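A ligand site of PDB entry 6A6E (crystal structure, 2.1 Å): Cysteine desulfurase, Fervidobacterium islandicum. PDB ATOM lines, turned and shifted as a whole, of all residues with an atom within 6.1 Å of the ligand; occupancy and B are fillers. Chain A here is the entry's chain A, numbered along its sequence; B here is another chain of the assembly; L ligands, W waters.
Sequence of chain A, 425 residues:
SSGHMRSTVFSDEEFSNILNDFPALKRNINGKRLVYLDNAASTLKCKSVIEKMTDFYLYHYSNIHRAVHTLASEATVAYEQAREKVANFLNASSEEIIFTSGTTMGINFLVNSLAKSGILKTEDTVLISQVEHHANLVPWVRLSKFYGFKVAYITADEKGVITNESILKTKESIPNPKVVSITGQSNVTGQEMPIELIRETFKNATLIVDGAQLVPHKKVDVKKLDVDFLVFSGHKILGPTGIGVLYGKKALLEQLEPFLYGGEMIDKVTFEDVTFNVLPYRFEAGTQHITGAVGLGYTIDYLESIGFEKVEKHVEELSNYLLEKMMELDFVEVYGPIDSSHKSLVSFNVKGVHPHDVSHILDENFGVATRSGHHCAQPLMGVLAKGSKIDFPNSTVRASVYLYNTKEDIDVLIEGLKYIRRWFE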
ATOM      1  N   ALA A  40      13.205  -6.783  31.653  1.00  0.00           N
ATOM      2  CA  ALA A  40      12.773  -5.605  30.973  1.00  0.00           C
ATOM      3  C   ALA A  40      12.231  -5.877  29.563  1.00  0.00           C
ATOM      4  O   ALA A  40      11.483  -5.090  29.027  1.00  0.00           O
ATOM      5  CB  ALA A  40      13.928  -4.684  30.922  1.00  0.00           C
ATOM      6  N   ALA A  41      12.596  -7.007  28.975  1.00  0.00           N
ATOM      7  CA  ALA A  41      12.052  -7.467  27.728  1.00  0.00           C
ATOM      8  C   ALA A  41      10.760  -8.277  27.937  1.00  0.00           C
ATOM      9  O   ALA A  41       9.814  -8.121  27.146  1.00  0.00           O
ATOM     10  CB  ALA A  41      13.090  -8.330  26.992  1.00  0.00           C
ATOM     11  N   SER A 101      -4.187  -5.391  23.116  1.00  0.00           N
ATOM     12  CA  SER A 101      -3.157  -6.417  22.825  1.00  0.00           C
ATOM     13  C   SER A 101      -1.823  -6.105  23.490  1.00  0.00           C
ATOM     14  O   SER A 101      -0.942  -6.970  23.545  1.00  0.00           O
ATOM     15  CB  SER A 101      -2.995  -6.604  21.345  1.00  0.00           C
ATOM     16  OG  SER A 101      -2.376  -5.457  20.765  1.00  0.00           O
ATOM     17  N   GLY A 102      -1.668  -4.876  24.032  1.00  0.00           N
ATOM     18  CA  GLY A 102      -0.363  -4.458  24.624  1.00  0.00           C
ATOM     19  C   GLY A 102      -0.156  -2.958  24.706  1.00  0.00           C
ATOM     20  O   GLY A 102      -0.997  -2.156  24.214  1.00  0.00           O
ATOM     21  N   THR A 103       0.959  -2.563  25.298  1.00  0.00           N
ATOM     22  CA  THR A 103       1.340  -1.162  25.323  1.00  0.00           C
ATOM     23  C   THR A 103       1.344  -0.541  23.920  1.00  0.00           C
ATOM     24  O   THR A 103       0.766   0.498  23.726  1.00  0.00           O
ATOM     25  CB  THR A 103       2.689  -0.991  25.920  1.00  0.00           C
ATOM     26  OG1 THR A 103       2.689  -1.494  27.257  1.00  0.00           O
ATOM     27  CG2 THR A 103       3.103   0.522  25.897  1.00  0.00           C
ATOM     28  N   THR A 104       2.045  -1.183  22.987  1.00  0.00           N
ATOM     29  CA  THR A 104       2.163  -0.680  21.649  1.00  0.00           C
ATOM     30  C   THR A 104       0.803  -0.370  21.040  1.00  0.00           C
ATOM     31  O   THR A 104       0.587   0.736  20.511  1.00  0.00           O
ATOM     32  CB  THR A 104       2.976  -1.630  20.769  1.00  0.00           C
ATOM     33  OG1 THR A 104       4.270  -1.835  21.352  1.00  0.00           O
ATOM     34  CG2 THR A 104       3.152  -1.082  19.342  1.00  0.00           C
ATOM     35  N   MET A 105      -0.124  -1.318  21.085  1.00  0.00           N
ATOM     36  CA  MET A 105      -1.481  -1.050  20.557  1.00  0.00           C
ATOM     37  C   MET A 105      -2.117   0.163  21.252  1.00  0.00           C
ATOM     38  O   MET A 105      -2.718   1.014  20.613  1.00  0.00           O
ATOM     39  CB  MET A 105      -2.410  -2.270  20.680  1.00  0.00           C
ATOM     40  CG  MET A 105      -3.914  -1.900  20.543  1.00  0.00           C
ATOM     41  SD  MET A 105      -5.038  -3.305  20.366  1.00  0.00           S
ATOM     42  CE  MET A 105      -6.664  -2.549  20.725  1.00  0.00           C
ATOM     43  N   HIS A 133      10.936   4.684  24.190  1.00  0.00           N
ATOM     44  CA  HIS A 133      10.808   3.467  23.433  1.00  0.00           C
ATOM     45  C   HIS A 133      10.103   3.760  22.093  1.00  0.00           C
ATOM     46  O   HIS A 133       9.288   4.670  21.969  1.00  0.00           O
ATOM     47  CB  HIS A 133      10.065   2.452  24.331  1.00  0.00           C
ATOM     48  CG  HIS A 133       9.988   1.053  23.765  1.00  0.00           C
ATOM     49  ND1 HIS A 133       9.192   0.736  22.668  1.00  0.00           N
ATOM     50  CD2 HIS A 133      10.511  -0.105  24.206  1.00  0.00           C
ATOM     51  CE1 HIS A 133       9.286  -0.554  22.427  1.00  0.00           C
ATOM     52  NE2 HIS A 133      10.096  -1.084  23.334  1.00  0.00           N
ATOM     53  N   ALA A 135       7.781   2.386  20.692  1.00  0.00           N
ATOM     54  CA  ALA A 135       6.291   2.314  20.850  1.00  0.00           C
ATOM     55  C   ALA A 135       5.617   3.638  21.189  1.00  0.00           C
ATOM     56  O   ALA A 135       4.450   3.885  20.816  1.00  0.00           O
ATOM     57  CB  ALA A 135       5.961   1.327  21.916  1.00  0.00           C
ATOM     58  N   ASN A 136       6.367   4.483  21.904  1.00  0.00           N
ATOM     59  CA  ASN A 136       5.923   5.852  22.243  1.00  0.00           C
ATOM     60  C   ASN A 136       6.704   6.923  21.467  1.00  0.00           C
ATOM     61  O   ASN A 136       6.857   8.077  21.921  1.00  0.00           O
ATOM     62  CB  ASN A 136       6.004   6.094  23.761  1.00  0.00           C
ATOM     63  CG  ASN A 136       5.125   7.275  24.193  1.00  0.00           C
ATOM     64  OD1 ASN A 136       4.107   7.554  23.569  1.00  0.00           O
ATOM     65  ND2 ASN A 136       5.514   7.940  25.292  1.00  0.00           N
ATOM     66  N   THR A 183       7.372   8.345  29.026  1.00  0.00           N
ATOM     67  CA  THR A 183       7.572   7.108  29.727  1.00  0.00           C
ATOM     68  C   THR A 183       7.490   7.318  31.229  1.00  0.00           C
ATOM     69  O   THR A 183       7.859   8.356  31.764  1.00  0.00           O
ATOM     70  CB  THR A 183       8.919   6.441  29.368  1.00  0.00           C
ATOM     71  OG1 THR A 183       8.985   5.189  30.022  1.00  0.00           O
ATOM     72  CG2 THR A 183      10.153   7.300  29.775  1.00  0.00           C
ATOM     73  N   GLN A 185       8.970   5.147  33.069  1.00  0.00           N
ATOM     74  CA  GLN A 185      10.333   4.717  33.413  1.00  0.00           C
ATOM     75  C   GLN A 185      11.014   4.163  32.166  1.00  0.00           C
ATOM     76  O   GLN A 185      10.411   3.312  31.469  1.00  0.00           O
ATOM     77  CB  GLN A 185      10.292   3.588  34.457  1.00  0.00           C
ATOM     78  CG  GLN A 185      11.661   2.983  34.788  1.00  0.00           C
ATOM     79  CD  GLN A 185      11.577   1.807  35.729  1.00  0.00           C
ATOM     80  OE1 GLN A 185      10.504   1.288  35.960  1.00  0.00           O
ATOM     81  NE2 GLN A 185      12.687   1.418  36.303  1.00  0.00           N
ATOM     82  N   SER A 186      12.243   4.606  31.894  1.00  0.00           N
ATOM     83  CA  SER A 186      12.990   4.213  30.705  1.00  0.00           C
ATOM     84  C   SER A 186      13.420   2.780  30.830  1.00  0.00           C
ATOM     85  O   SER A 186      13.880   2.332  31.892  1.00  0.00           O
ATOM     86  CB  SER A 186      14.194   5.131  30.440  1.00  0.00           C
ATOM     87  OG  SER A 186      15.088   4.602  29.457  1.00  0.00           O
ATOM     88  N   ASN A 187      13.246   2.069  29.715  1.00  0.00           N
ATOM     89  CA  ASN A 187      13.697   0.697  29.540  1.00  0.00           C
ATOM     90  C   ASN A 187      15.215   0.608  29.261  1.00  0.00           C
ATOM     91  O   ASN A 187      15.707  -0.499  29.141  1.00  0.00           O
ATOM     92  CB  ASN A 187      12.949   0.005  28.388  1.00  0.00           C
ATOM     93  CG  ASN A 187      13.334   0.531  27.028  1.00  0.00           C
ATOM     94  OD1 ASN A 187      13.358   1.722  26.828  1.00  0.00           O
ATOM     95  ND2 ASN A 187      13.616  -0.363  26.064  1.00  0.00           N
ATOM     96  N   ASP A 210       3.439   6.087  29.269  1.00  0.00           N
ATOM     97  CA  ASP A 210       3.868   4.775  28.938  1.00  0.00           C
ATOM     98  C   ASP A 210       4.419   4.114  30.172  1.00  0.00           C
ATOM     99  O   ASP A 210       5.564   4.333  30.556  1.00  0.00           O
ATOM    100  CB  ASP A 210       4.871   4.808  27.745  1.00  0.00           C
ATOM    101  CG  ASP A 210       5.501   3.430  27.413  1.00  0.00           C
ATOM    102  OD1 ASP A 210       5.144   2.461  28.064  1.00  0.00           O
ATOM    103  OD2 ASP A 210       6.404   3.355  26.521  1.00  0.00           O
ATOM    104  N   GLY A 211       3.612   3.220  30.705  1.00  0.00           N
ATOM    105  CA  GLY A 211       3.826   2.560  31.958  1.00  0.00           C
ATOM    106  C   GLY A 211       4.446   1.185  31.864  1.00  0.00           C
ATOM    107  O   GLY A 211       4.525   0.481  32.910  1.00  0.00           O
ATOM    108  N   ALA A 212       4.927   0.782  30.677  1.00  0.00           N
ATOM    109  CA  ALA A 212       5.286  -0.667  30.490  1.00  0.00           C
ATOM    110  C   ALA A 212       6.311  -1.182  31.489  1.00  0.00           C
ATOM    111  O   ALA A 212       6.243  -2.347  31.924  1.00  0.00           O
ATOM    112  CB  ALA A 212       5.749  -0.959  29.060  1.00  0.00           C
ATOM    113  N   GLN A 213       7.315  -0.349  31.815  1.00  0.00           N
ATOM    114  CA  GLN A 213       8.403  -0.760  32.727  1.00  0.00           C
ATOM    115  C   GLN A 213       8.070  -0.408  34.179  1.00  0.00           C
ATOM    116  O   GLN A 213       8.603  -1.042  35.085  1.00  0.00           O
ATOM    117  CB  GLN A 213       9.727  -0.089  32.443  1.00  0.00           C
ATOM    118  CG  GLN A 213      10.431  -0.473  31.226  1.00  0.00           C
ATOM    119  CD  GLN A 213      10.849  -1.923  31.199  1.00  0.00           C
ATOM    120  OE1 GLN A 213      11.193  -2.528  32.240  1.00  0.00           O
ATOM    121  NE2 GLN A 213      10.808  -2.500  29.994  1.00  0.00           N
ATOM    122  N   SER A 233       1.672  -3.450  29.532  1.00  0.00           N
ATOM    123  CA  SER A 233       1.585  -4.764  28.910  1.00  0.00           C
ATOM    124  C   SER A 233       1.603  -5.836  29.988  1.00  0.00           C
ATOM    125  O   SER A 233       2.457  -5.821  30.936  1.00  0.00           O
ATOM    126  CB  SER A 233       2.777  -5.020  27.983  1.00  0.00           C
ATOM    127  OG  SER A 233       2.857  -4.098  26.887  1.00  0.00           O
ATOM    128  N   HIS A 235       2.619  -8.968  29.758  1.00  0.00           N
ATOM    129  CA  HIS A 235       3.734  -9.961  29.706  1.00  0.00           C
ATOM    130  C   HIS A 235       4.942  -9.519  30.538  1.00  0.00           C
ATOM    131  O   HIS A 235       5.768 -10.382  30.880  1.00  0.00           O
ATOM    132  CB  HIS A 235       4.208 -10.365  28.298  1.00  0.00           C
ATOM    133  CG  HIS A 235       4.833  -9.236  27.526  1.00  0.00           C
ATOM    134  ND1 HIS A 235       6.208  -9.076  27.437  1.00  0.00           N
ATOM    135  CD2 HIS A 235       4.281  -8.251  26.776  1.00  0.00           C
ATOM    136  CE1 HIS A 235       6.457  -7.992  26.708  1.00  0.00           C
ATOM    137  NE2 HIS A 235       5.299  -7.469  26.311  1.00  0.00           N
ATOM    138  N   LYS A 236       5.008  -8.211  30.839  1.00  0.00           N
ATOM    139  CA  LYS A 236       6.006  -7.636  31.698  1.00  0.00           C
ATOM    140  C   LYS A 236       5.724  -7.635  33.198  1.00  0.00           C
ATOM    141  O   LYS A 236       6.613  -7.287  33.978  1.00  0.00           O
ATOM    142  CB  LYS A 236       6.434  -6.225  31.244  1.00  0.00           C
ATOM    143  CG  LYS A 236       7.188  -6.250  29.909  1.00  0.00           C
ATOM    144  CD  LYS A 236       7.702  -4.872  29.530  1.00  0.00           C
ATOM    145  CE  LYS A 236       8.270  -4.891  28.130  1.00  0.00           C
ATOM    146  NZ  LYS A 236       8.598  -3.488  27.722  1.00  0.00           N
ATOM    147  N   ASN B  63      11.101 -12.898  25.294  1.00  0.00           N
ATOM    148  CA  ASN B  63      10.772 -12.068  24.137  1.00  0.00           C
ATOM    149  C   ASN B  63      11.688 -12.473  22.938  1.00  0.00           C
ATOM    150  O   ASN B  63      12.745 -13.090  23.146  1.00  0.00           O
ATOM    151  CB  ASN B  63      10.829 -10.572  24.479  1.00  0.00           C
ATOM    152  CG  ASN B  63       9.783  -9.758  23.700  1.00  0.00           C
ATOM    153  OD1 ASN B  63       9.381 -10.195  22.610  1.00  0.00           O
ATOM    154  ND2 ASN B  63       9.278  -8.653  24.273  1.00  0.00           N
ATOM    155  N   ALA B 285       3.736  -4.822  14.987  1.00  0.00           N
ATOM    156  CA  ALA B 285       4.198  -3.767  15.897  1.00  0.00           C
ATOM    157  C   ALA B 285       4.265  -4.223  17.342  1.00  0.00           C
ATOM    158  O   ALA B 285       3.241  -4.608  17.956  1.00  0.00           O
ATOM    159  CB  ALA B 285       3.270  -2.600  15.785  1.00  0.00           C
ATOM    160  N   GLY B 286       5.463  -4.186  17.892  1.00  0.00           N
ATOM    161  CA  GLY B 286       5.646  -4.569  19.273  1.00  0.00           C
ATOM    162  C   GLY B 286       5.417  -6.061  19.570  1.00  0.00           C
ATOM    163  O   GLY B 286       5.329  -6.901  18.642  1.00  0.00           O
ATOM    164  N   THR B 287       5.394  -6.394  20.845  1.00  0.00           N
ATOM    165  CA  THR B 287       5.297  -7.805  21.235  1.00  0.00           C
ATOM    166  C   THR B 287       3.919  -8.371  20.888  1.00  0.00           C
ATOM    167  O   THR B 287       2.878  -7.914  21.364  1.00  0.00           O
ATOM    168  CB  THR B 287       5.637  -7.987  22.730  1.00  0.00           C
ATOM    169  OG1 THR B 287       6.824  -7.236  23.057  1.00  0.00           O
ATOM    170  CG2 THR B 287       5.800  -9.442  23.054  1.00  0.00           C
ATOM    171  N   GLN B 288       3.933  -9.422  20.079  1.00  0.00           N
ATOM    172  CA  GLN B 288       2.731 -10.064  19.602  1.00  0.00           C
ATOM    173  C   GLN B 288       2.272 -11.111  20.645  1.00  0.00           C
ATOM    174  O   GLN B 288       2.848 -11.267  21.772  1.00  0.00           O
ATOM    175  CB  GLN B 288       3.011 -10.716  18.224  1.00  0.00           C
ATOM    176  CG  GLN B 288       3.314  -9.736  17.112  1.00  0.00           C
ATOM    177  CD  GLN B 288       2.236  -8.709  17.015  1.00  0.00           C
ATOM    178  OE1 GLN B 288       1.148  -9.053  16.742  1.00  0.00           O
ATOM    179  NE2 GLN B 288       2.573  -7.426  17.285  1.00  0.00           N
HETATM  180  N1  LIG L   1       7.603   1.108  26.388  1.00  0.00           N
HETATM  181  C1  LIG L   1       8.458   0.688  27.281  1.00  0.00           C
HETATM  182  C2  LIG L   1       9.176   1.666  28.156  1.00  0.00           C
HETATM  183  C3  LIG L   1       8.701  -0.753  27.360  1.00  0.00           C
HETATM  184  O1  LIG L   1       9.596  -1.178  28.243  1.00  0.00           O
HETATM  185  C4  LIG L   1       7.956  -1.681  26.513  1.00  0.00           C
HETATM  186  C5  LIG L   1       8.080  -3.123  26.593  1.00  0.00           C
HETATM  187  C6  LIG L   1       7.052  -1.094  25.520  1.00  0.00           C
HETATM  188  C7  LIG L   1       6.944   0.262  25.541  1.00  0.00           C
HETATM  189  C8  LIG L   1       6.283  -1.954  24.513  1.00  0.00           C
HETATM  190  O2  LIG L   1       5.537  -3.073  24.962  1.00  0.00           O
HETATM  191  P1  LIG L   1       4.892  -4.244  24.042  1.00  0.00           P
HETATM  192  O3  LIG L   1       3.837  -3.646  23.194  1.00  0.00           O
HETATM  193  O4  LIG L   1       6.104  -4.804  23.357  1.00  0.00           O
HETATM  194  O5  LIG L   1       4.304  -5.109  25.118  1.00  0.00           O
HETATM  195  O   HOH W   1       2.237  -5.510  22.446  1.00  0.00           O
HETATM  196  O   HOH W   2      10.951   4.452  27.921  1.00  0.00           O
HETATM  197  O   HOH W   3       1.726  -7.159  24.742  1.00  0.00           O
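The side-chain amide nitrogen (NE2) of Gln 213 lies within hydrogen-bond range of an oxygen (O1) of the ligand (2.5 Å).
The side-chain carboxylate (OD2) of Asp 210 is in hydrogen-bond range of a nitrogen (N1) of the ligand, at 2.6 Å.
A carbon (C5) of the ligand is bonded to the side-chain amino group of Lys 236.
N of Thr 287 of chain B is in hydrogen-bond range of O4 of the ligand.
The backbone NH (N) of Thr 104 sits at hydrogen-bond distance from an oxygen (O3) of the ligand (3.1 Å).
OG1 of Thr 104 sits at hydrogen-bond distance from O3 of the ligand (2.6 Å).
OG1 of Thr 287 of chain B is in hydrogen-bond range of O4 of the ligand.
A ring nitrogen (NE2) of His 235 sits at hydrogen-bond distance from an oxygen (O5) of the ligand (2.8 Å).
OG of Ser 233 is in hydrogen-bond range of O5 of the ligand (2.5 Å).
NE2 of Gln 213 sits at hydrogen-bond distance from O of Ala 40 (2.8 Å).
The side-chain hydroxyl of Ser 233 is in hydrogen-bond range of the side-chain hydroxyl of Thr 103 (2.6 Å).
The side-chain carboxylate (OD1) of Asp 210 lies within hydrogen-bond range of the backbone NH (N) of Ala 212 (3.1 Å).
The side-chain amide oxygen of Gln 185 sits close to the backbone carbonyl oxygen of Gln 213.
ND1 of His 133 is in hydrogen-bond range of N of Ala 135 (2.9 Å).
The side-chain amide nitrogen (ND2) of Asn 63 of chain B is in hydrogen-bond range of the side-chain hydroxyl (OG1) of Thr 287 of chain B (3.1 Å).
The backbone carbonyl oxygen (O) of Gln 185 sits at hydrogen-bond distance from the side-chain hydroxyl (OG1) of Thr 183, at 2.8 Å.
NZ of Lys 236 sits close to NE2 of Gln 213 (3.3 Å).
CB of Thr 103 touches O2 of the ligand, 3.7 Å away.
His 133 touches the ligand.
Ala 135 touches the ligand (CB to C7, 3.9 Å).
Thr 183 touches the ligand (OG1 to C2, 3.99 Å).
Gln 185 touches the ligand (O to C2, 3.9 Å).
CB of Asn 187 touches O1 of the ligand, 3.6 Å away.
Ala 212 touches the ligand (CB to C3, 3.4 Å).
Hydrophobic or aromatic side chains within 4 Å of the ligand: His 133, Ala 135, Ala 212 and His 235.
14 residues have an atom within 4 Å of the ligand: Thr 103, Thr 104, His 133, Ala 135, Thr 183, Gln 185, Asn 187, Asp 210, Ala 212, Gln 213, Ser 233, His 235, Lys 236 and Thr 287 of chain B.
Water W1 bridges O3 of the ligand and O of Thr 287 of chain B.
Water W3 lies within hydrogen-bond range of O of Ser 101 and O5 of the ligand.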
